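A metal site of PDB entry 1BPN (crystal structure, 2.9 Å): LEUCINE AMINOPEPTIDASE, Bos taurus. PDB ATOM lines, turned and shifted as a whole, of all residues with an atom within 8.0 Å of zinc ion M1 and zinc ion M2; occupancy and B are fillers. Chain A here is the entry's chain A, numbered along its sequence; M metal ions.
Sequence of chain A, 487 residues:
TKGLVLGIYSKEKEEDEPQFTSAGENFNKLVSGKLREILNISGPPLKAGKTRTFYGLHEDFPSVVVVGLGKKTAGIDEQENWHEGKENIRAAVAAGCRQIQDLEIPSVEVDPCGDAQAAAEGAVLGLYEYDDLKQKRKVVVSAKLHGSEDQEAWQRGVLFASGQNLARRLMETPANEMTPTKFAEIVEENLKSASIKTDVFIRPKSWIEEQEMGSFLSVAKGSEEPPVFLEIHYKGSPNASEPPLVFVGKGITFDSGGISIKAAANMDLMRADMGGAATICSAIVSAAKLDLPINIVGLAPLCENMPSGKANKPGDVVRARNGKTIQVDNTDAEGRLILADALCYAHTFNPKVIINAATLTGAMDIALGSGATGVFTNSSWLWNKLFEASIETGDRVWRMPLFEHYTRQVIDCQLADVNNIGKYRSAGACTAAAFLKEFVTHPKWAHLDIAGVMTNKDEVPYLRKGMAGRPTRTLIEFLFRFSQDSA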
ATOM      1  N   VAL A 219      -5.054  24.722  -9.425  1.00  0.00           N
ATOM      2  CA  VAL A 219      -4.325  24.442 -10.614  1.00  0.00           C
ATOM      3  C   VAL A 219      -4.837  23.182 -11.277  1.00  0.00           C
ATOM      4  O   VAL A 219      -5.061  23.187 -12.482  1.00  0.00           O
ATOM      5  CB  VAL A 219      -2.862  24.300 -10.264  1.00  0.00           C
ATOM      6  CG1 VAL A 219      -2.091  24.249 -11.577  1.00  0.00           C
ATOM      7  CG2 VAL A 219      -2.360  25.467  -9.432  1.00  0.00           C
ATOM      8  N   LYS A 250       7.921  20.375  -8.391  1.00  0.00           N
ATOM      9  CA  LYS A 250       6.717  20.619  -9.154  1.00  0.00           C
ATOM     10  C   LYS A 250       6.535  19.605 -10.275  1.00  0.00           C
ATOM     11  O   LYS A 250       7.448  19.241 -11.018  1.00  0.00           O
ATOM     12  CB  LYS A 250       6.792  22.089  -9.615  1.00  0.00           C
ATOM     13  CG  LYS A 250       7.344  22.538 -10.954  1.00  0.00           C
ATOM     14  CD  LYS A 250       6.296  23.337 -11.677  1.00  0.00           C
ATOM     15  CE  LYS A 250       6.990  24.311 -12.567  1.00  0.00           C
ATOM     16  NZ  LYS A 250       6.200  24.498 -13.743  1.00  0.00           N
ATOM     17  N   GLY A 251       5.311  19.087 -10.323  1.00  0.00           N
ATOM     18  CA  GLY A 251       4.975  18.026 -11.243  1.00  0.00           C
ATOM     19  C   GLY A 251       3.788  18.296 -12.154  1.00  0.00           C
ATOM     20  O   GLY A 251       2.777  17.586 -12.099  1.00  0.00           O
ATOM     21  N   ILE A 252       3.896  19.304 -13.017  1.00  0.00           N
ATOM     22  CA  ILE A 252       2.850  19.548 -14.024  1.00  0.00           C
ATOM     23  C   ILE A 252       3.170  18.531 -15.129  1.00  0.00           C
ATOM     24  O   ILE A 252       4.248  18.646 -15.747  1.00  0.00           O
ATOM     25  CB  ILE A 252       2.943  21.011 -14.518  1.00  0.00           C
ATOM     26  CG1 ILE A 252       2.783  22.038 -13.379  1.00  0.00           C
ATOM     27  CG2 ILE A 252       1.892  21.182 -15.578  1.00  0.00           C
ATOM     28  CD1 ILE A 252       1.507  22.091 -12.496  1.00  0.00           C
ATOM     29  N   PHE A 254       1.853  18.070 -18.018  1.00  0.00           N
ATOM     30  CA  PHE A 254       1.825  18.903 -19.170  1.00  0.00           C
ATOM     31  C   PHE A 254       1.337  20.287 -18.779  1.00  0.00           C
ATOM     32  O   PHE A 254       0.310  20.367 -18.109  1.00  0.00           O
ATOM     33  CB  PHE A 254       0.907  18.343 -20.220  1.00  0.00           C
ATOM     34  CG  PHE A 254       1.190  19.080 -21.519  1.00  0.00           C
ATOM     35  CD1 PHE A 254       2.338  18.784 -22.215  1.00  0.00           C
ATOM     36  CD2 PHE A 254       0.385  20.125 -21.897  1.00  0.00           C
ATOM     37  CE1 PHE A 254       2.739  19.605 -23.229  1.00  0.00           C
ATOM     38  CE2 PHE A 254       0.775  20.937 -22.945  1.00  0.00           C
ATOM     39  CZ  PHE A 254       1.964  20.688 -23.599  1.00  0.00           C
ATOM     40  N   ASP A 255       2.129  21.302 -19.197  1.00  0.00           N
ATOM     41  CA  ASP A 255       1.798  22.738 -19.066  1.00  0.00           C
ATOM     42  C   ASP A 255       1.392  23.442 -20.382  1.00  0.00           C
ATOM     43  O   ASP A 255       2.213  23.775 -21.222  1.00  0.00           O
ATOM     44  CB  ASP A 255       2.966  23.545 -18.496  1.00  0.00           C
ATOM     45  CG  ASP A 255       2.572  24.882 -17.830  1.00  0.00           C
ATOM     46  OD1 ASP A 255       1.457  25.404 -18.041  1.00  0.00           O
ATOM     47  OD2 ASP A 255       3.365  25.390 -17.021  1.00  0.00           O
ATOM     48  N   SER A 256       0.122  23.717 -20.618  1.00  0.00           N
ATOM     49  CA  SER A 256      -0.335  24.477 -21.775  1.00  0.00           C
ATOM     50  C   SER A 256      -0.521  25.972 -21.432  1.00  0.00           C
ATOM     51  O   SER A 256      -1.027  26.763 -22.232  1.00  0.00           O
ATOM     52  CB  SER A 256      -1.663  23.935 -22.231  1.00  0.00           C
ATOM     53  OG  SER A 256      -2.718  24.231 -21.303  1.00  0.00           O
ATOM     54  N   GLY A 257      -0.217  26.331 -20.175  1.00  0.00           N
ATOM     55  CA  GLY A 257      -0.415  27.678 -19.703  1.00  0.00           C
ATOM     56  C   GLY A 257      -1.785  27.896 -19.124  1.00  0.00           C
ATOM     57  O   GLY A 257      -1.932  28.810 -18.315  1.00  0.00           O
ATOM     58  N   GLY A 258      -2.775  27.082 -19.515  1.00  0.00           N
ATOM     59  CA  GLY A 258      -4.151  27.221 -19.073  1.00  0.00           C
ATOM     60  C   GLY A 258      -4.899  28.278 -19.876  1.00  0.00           C
ATOM     61  O   GLY A 258      -4.800  28.302 -21.101  1.00  0.00           O
ATOM     62  N   SER A 260      -4.283  31.447 -19.362  1.00  0.00           N
ATOM     63  CA  SER A 260      -3.153  32.273 -19.751  1.00  0.00           C
ATOM     64  C   SER A 260      -2.153  31.403 -20.526  1.00  0.00           C
ATOM     65  O   SER A 260      -0.973  31.319 -20.190  1.00  0.00           O
ATOM     66  CB  SER A 260      -2.570  32.905 -18.482  1.00  0.00           C
ATOM     67  OG  SER A 260      -3.385  34.003 -18.049  1.00  0.00           O
ATOM     68  N   LYS A 262      -0.252  29.259 -23.466  1.00  0.00           N
ATOM     69  CA  LYS A 262       0.973  29.259 -24.220  1.00  0.00           C
ATOM     70  C   LYS A 262       0.789  29.324 -25.726  1.00  0.00           C
ATOM     71  O   LYS A 262      -0.264  29.051 -26.278  1.00  0.00           O
ATOM     72  CB  LYS A 262       1.807  28.010 -23.861  1.00  0.00           C
ATOM     73  CG  LYS A 262       2.201  27.917 -22.378  1.00  0.00           C
ATOM     74  CD  LYS A 262       3.119  26.733 -22.151  1.00  0.00           C
ATOM     75  CE  LYS A 262       3.727  26.694 -20.744  1.00  0.00           C
ATOM     76  NZ  LYS A 262       4.510  27.886 -20.460  1.00  0.00           N
ATOM     77  N   MET A 270       6.553  20.908 -22.776  1.00  0.00           N
ATOM     78  CA  MET A 270       5.954  21.201 -21.470  1.00  0.00           C
ATOM     79  C   MET A 270       5.598  19.992 -20.672  1.00  0.00           C
ATOM     80  O   MET A 270       5.364  20.090 -19.473  1.00  0.00           O
ATOM     81  CB  MET A 270       4.736  22.070 -21.615  1.00  0.00           C
ATOM     82  CG  MET A 270       5.092  23.468 -22.064  1.00  0.00           C
ATOM     83  SD  MET A 270       6.663  24.184 -21.475  1.00  0.00           S
ATOM     84  CE  MET A 270       6.547  24.232 -19.705  1.00  0.00           C
ATOM     85  N   ALA A 272       7.772  18.245 -19.876  1.00  0.00           N
ATOM     86  CA  ALA A 272       8.842  18.153 -18.925  1.00  0.00           C
ATOM     87  C   ALA A 272       8.786  19.271 -17.918  1.00  0.00           C
ATOM     88  O   ALA A 272       9.806  19.692 -17.369  1.00  0.00           O
ATOM     89  CB  ALA A 272      10.168  18.210 -19.607  1.00  0.00           C
ATOM     90  N   ASP A 273       7.552  19.750 -17.654  1.00  0.00           N
ATOM     91  CA  ASP A 273       7.328  20.721 -16.579  1.00  0.00           C
ATOM     92  C   ASP A 273       7.091  19.976 -15.271  1.00  0.00           C
ATOM     93  O   ASP A 273       6.916  20.590 -14.215  1.00  0.00           O
ATOM     94  CB  ASP A 273       6.144  21.586 -16.966  1.00  0.00           C
ATOM     95  CG  ASP A 273       6.111  22.914 -16.236  1.00  0.00           C
ATOM     96  OD1 ASP A 273       7.151  23.559 -16.111  1.00  0.00           O
ATOM     97  OD2 ASP A 273       5.031  23.289 -15.793  1.00  0.00           O
ATOM     98  N   MET A 274       7.065  18.623 -15.341  1.00  0.00           N
ATOM     99  CA  MET A 274       7.146  17.704 -14.202  1.00  0.00           C
ATOM    100  C   MET A 274       8.607  17.338 -13.903  1.00  0.00           C
ATOM    101  O   MET A 274       8.871  16.387 -13.165  1.00  0.00           O
ATOM    102  CB  MET A 274       6.406  16.385 -14.432  1.00  0.00           C
ATOM    103  CG  MET A 274       6.606  15.702 -15.777  1.00  0.00           C
ATOM    104  SD  MET A 274       8.277  15.294 -16.334  1.00  0.00           S
ATOM    105  CE  MET A 274       8.276  14.124 -14.998  1.00  0.00           C
ATOM    106  N   ASN A 305      -1.897  21.458 -16.295  1.00  0.00           N
ATOM    107  CA  ASN A 305      -2.436  22.810 -16.461  1.00  0.00           C
ATOM    108  C   ASN A 305      -3.080  22.988 -17.843  1.00  0.00           C
ATOM    109  O   ASN A 305      -2.449  23.097 -18.892  1.00  0.00           O
ATOM    110  CB  ASN A 305      -1.290  23.779 -16.193  1.00  0.00           C
ATOM    111  CG  ASN A 305      -1.762  25.206 -15.974  1.00  0.00           C
ATOM    112  OD1 ASN A 305      -1.110  26.118 -16.451  1.00  0.00           O
ATOM    113  ND2 ASN A 305      -2.891  25.452 -15.307  1.00  0.00           N
ATOM    114  N   ASN A 330      -1.974  35.243 -13.706  1.00  0.00           N
ATOM    115  CA  ASN A 330      -1.498  34.499 -14.837  1.00  0.00           C
ATOM    116  C   ASN A 330      -1.450  33.050 -14.402  1.00  0.00           C
ATOM    117  O   ASN A 330      -0.682  32.645 -13.534  1.00  0.00           O
ATOM    118  CB  ASN A 330      -0.126  35.024 -15.230  1.00  0.00           C
ATOM    119  CG  ASN A 330       0.428  34.404 -16.502  1.00  0.00           C
ATOM    120  OD1 ASN A 330       0.622  33.201 -16.535  1.00  0.00           O
ATOM    121  ND2 ASN A 330       0.687  35.152 -17.581  1.00  0.00           N
ATOM    122  N   THR A 331      -2.292  32.288 -15.113  1.00  0.00           N
ATOM    123  CA  THR A 331      -2.525  30.845 -14.984  1.00  0.00           C
ATOM    124  C   THR A 331      -1.302  30.000 -15.392  1.00  0.00           C
ATOM    125  O   THR A 331      -1.210  28.816 -15.089  1.00  0.00           O
ATOM    126  CB  THR A 331      -3.828  30.616 -15.833  1.00  0.00           C
ATOM    127  OG1 THR A 331      -4.829  31.319 -15.110  1.00  0.00           O
ATOM    128  CG2 THR A 331      -4.412  29.219 -15.935  1.00  0.00           C
ATOM    129  N   ASP A 332      -0.287  30.563 -16.082  1.00  0.00           N
ATOM    130  CA  ASP A 332       0.959  29.878 -16.392  1.00  0.00           C
ATOM    131  C   ASP A 332       1.911  30.011 -15.209  1.00  0.00           C
ATOM    132  O   ASP A 332       2.843  29.248 -14.980  1.00  0.00           O
ATOM    133  CB  ASP A 332       1.532  30.525 -17.648  1.00  0.00           C
ATOM    134  CG  ASP A 332       2.294  29.661 -18.644  1.00  0.00           C
ATOM    135  OD1 ASP A 332       2.403  28.460 -18.417  1.00  0.00           O
ATOM    136  OD2 ASP A 332       2.766  30.190 -19.640  1.00  0.00           O
ATOM    137  N   ALA A 333       1.753  30.983 -14.321  1.00  0.00           N
ATOM    138  CA  ALA A 333       2.523  30.995 -13.095  1.00  0.00           C
ATOM    139  C   ALA A 333       1.890  29.940 -12.126  1.00  0.00           C
ATOM    140  O   ALA A 333       1.437  30.289 -11.040  1.00  0.00           O
ATOM    141  CB  ALA A 333       2.431  32.423 -12.577  1.00  0.00           C
ATOM    142  N   GLU A 334       1.799  28.641 -12.443  1.00  0.00           N
ATOM    143  CA  GLU A 334       1.132  27.645 -11.596  1.00  0.00           C
ATOM    144  C   GLU A 334       2.021  26.730 -10.766  1.00  0.00           C
ATOM    145  O   GLU A 334       1.591  26.085  -9.823  1.00  0.00           O
ATOM    146  CB  GLU A 334       0.235  26.785 -12.473  1.00  0.00           C
ATOM    147  CG  GLU A 334       0.811  25.604 -13.245  1.00  0.00           C
ATOM    148  CD  GLU A 334       1.999  25.968 -14.143  1.00  0.00           C
ATOM    149  OE1 GLU A 334       1.793  26.731 -15.117  1.00  0.00           O
ATOM    150  OE2 GLU A 334       3.112  25.498 -13.875  1.00  0.00           O
ATOM    151  N   GLY A 335       3.273  26.619 -11.155  1.00  0.00           N
ATOM    152  CA  GLY A 335       4.259  25.871 -10.418  1.00  0.00           C
ATOM    153  C   GLY A 335       4.438  26.558  -9.106  1.00  0.00           C
ATOM    154  O   GLY A 335       4.417  25.857  -8.128  1.00  0.00           O
ATOM    155  N   ARG A 336       4.522  27.907  -9.077  1.00  0.00           N
ATOM    156  CA  ARG A 336       4.572  28.693  -7.845  1.00  0.00           C
ATOM    157  C   ARG A 336       3.415  28.285  -6.903  1.00  0.00           C
ATOM    158  O   ARG A 336       3.587  28.142  -5.682  1.00  0.00           O
ATOM    159  CB  ARG A 336       4.419  30.231  -8.078  1.00  0.00           C
ATOM    160  CG  ARG A 336       4.295  30.907  -9.454  1.00  0.00           C
ATOM    161  CD  ARG A 336       5.644  31.261 -10.130  1.00  0.00           C
ATOM    162  NE  ARG A 336       5.840  31.043 -11.598  1.00  0.00           N
ATOM    163  CZ  ARG A 336       5.681  29.879 -12.305  1.00  0.00           C
ATOM    164  NH1 ARG A 336       5.206  28.728 -11.854  1.00  0.00           N
ATOM    165  NH2 ARG A 336       5.960  29.861 -13.596  1.00  0.00           N
ATOM    166  N   ILE A 338       1.505  25.385  -7.049  1.00  0.00           N
ATOM    167  CA  ILE A 338       1.538  23.950  -6.805  1.00  0.00           C
ATOM    168  C   ILE A 338       2.513  23.751  -5.639  1.00  0.00           C
ATOM    169  O   ILE A 338       2.195  23.018  -4.695  1.00  0.00           O
ATOM    170  CB  ILE A 338       1.949  23.277  -8.206  1.00  0.00           C
ATOM    171  CG1 ILE A 338       1.117  22.077  -8.334  1.00  0.00           C
ATOM    172  CG2 ILE A 338       3.334  22.692  -8.344  1.00  0.00           C
ATOM    173  CD1 ILE A 338      -0.262  22.521  -8.748  1.00  0.00           C
ATOM    174  N   ALA A 358      12.256  22.941  -9.461  1.00  0.00           N
ATOM    175  CA  ALA A 358      11.195  23.150 -10.379  1.00  0.00           C
ATOM    176  C   ALA A 358      11.626  23.804 -11.641  1.00  0.00           C
ATOM    177  O   ALA A 358      12.382  24.759 -11.609  1.00  0.00           O
ATOM    178  CB  ALA A 358      10.134  24.020  -9.740  1.00  0.00           C
ATOM    179  N   THR A 359      11.047  23.320 -12.739  1.00  0.00           N
ATOM    180  CA  THR A 359      11.160  23.948 -14.058  1.00  0.00           C
ATOM    181  C   THR A 359      10.237  25.165 -13.953  1.00  0.00           C
ATOM    182  O   THR A 359       9.179  25.217 -14.591  1.00  0.00           O
ATOM    183  CB  THR A 359      10.693  22.918 -15.098  1.00  0.00           C
ATOM    184  OG1 THR A 359       9.452  22.414 -14.599  1.00  0.00           O
ATOM    185  CG2 THR A 359      11.670  21.798 -15.327  1.00  0.00           C
ATOM    186  N   LEU A 360      10.603  26.135 -13.109  1.00  0.00           N
ATOM    187  CA  LEU A 360       9.700  27.198 -12.768  1.00  0.00           C
ATOM    188  C   LEU A 360       9.471  28.351 -13.727  1.00  0.00           C
ATOM    189  O   LEU A 360       8.311  28.707 -13.935  1.00  0.00           O
ATOM    190  CB  LEU A 360      10.085  27.824 -11.440  1.00  0.00           C
ATOM    191  CG  LEU A 360       9.223  27.771 -10.164  1.00  0.00           C
ATOM    192  CD1 LEU A 360       9.495  29.050  -9.397  1.00  0.00           C
ATOM    193  CD2 LEU A 360       7.748  27.778 -10.437  1.00  0.00           C
ATOM    194  N   THR A 361      10.504  28.961 -14.340  1.00  0.00           N
ATOM    195  CA  THR A 361      10.389  30.164 -15.172  1.00  0.00           C
ATOM    196  C   THR A 361      11.348  30.086 -16.347  1.00  0.00           C
ATOM    197  O   THR A 361      12.498  29.676 -16.239  1.00  0.00           O
ATOM    198  CB  THR A 361      10.755  31.506 -14.381  1.00  0.00           C
ATOM    199  OG1 THR A 361      12.143  31.445 -14.011  1.00  0.00           O
ATOM    200  CG2 THR A 361       9.968  31.708 -13.114  1.00  0.00           C
HETATM  201 ZN    ZN M   1       4.752  25.371 -15.295  1.00  0.00          ZN
HETATM  202 ZN    ZN M   2       3.243  27.555 -16.568  1.00  0.00          ZN
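The side-chain carboxylate (OD1) of Asp 255 lies within hydrogen-bond range of the backbone NH (N) of Gly 257 (2.9 Å).
OD1 of Asn 305 lies close to OE1 of Glu 334 (3.3 Å).
The side-chain carboxylate of Asp 273 sits at hydrogen-bond distance from the side-chain hydroxyl of Thr 359.
The side-chain amide oxygen (OD1) of Asn 330 is in hydrogen-bond range of the backbone NH (N) of Asp 332, at 2.8 Å.
The backbone NH of Asp 332 lies within hydrogen-bond range of the backbone carbonyl oxygen of Gly 257 (3.3 Å).
The backbone NH (N) of Ile 252 lies within hydrogen-bond range of the backbone carbonyl oxygen (O) of Asp 273 (3.5 Å).
The side-chain amide oxygen (OD1) of Asn 305 lies close to the side-chain carboxylate (OD1) of Asp 255 (3.1 Å).
The backbone NH of Asp 255 is in hydrogen-bond range of the backbone carbonyl oxygen of Met 270 (3.5 Å).
The nearest printed residue that does not touch zinc ion M1 is Ile 252 (4.3 Å).
Within 4 Å of zinc ion M2: Asp 255, Asp 332 and Glu 334.
The nearest printed residue that does not touch zinc ion M2 is Lys 262 (4.1 Å).
Zinc ion M1 is bound by the side-chain carboxylate (OD2) of Asp 273 (2.2 Å), the side-chain carboxylate (OE2) of Glu 334 (2.2 Å), the side-chain carboxylate (OD2) of Asp 255 (2.2 Å) and the side-chain amino group (NZ) of Lys 250 (2.3 Å).
Zinc ion M2 is bound by the side-chain carboxylate of Glu 334 (2.2 Å), the side-chain carboxylate of Asp 255 (2.2 Å), the side-chain carboxylate of Asp 332 (2.2 Å) and the backbone carbonyl oxygen of Asp 332 (2.4 Å).
Zinc ion M2 has four donor atoms within binding distance.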
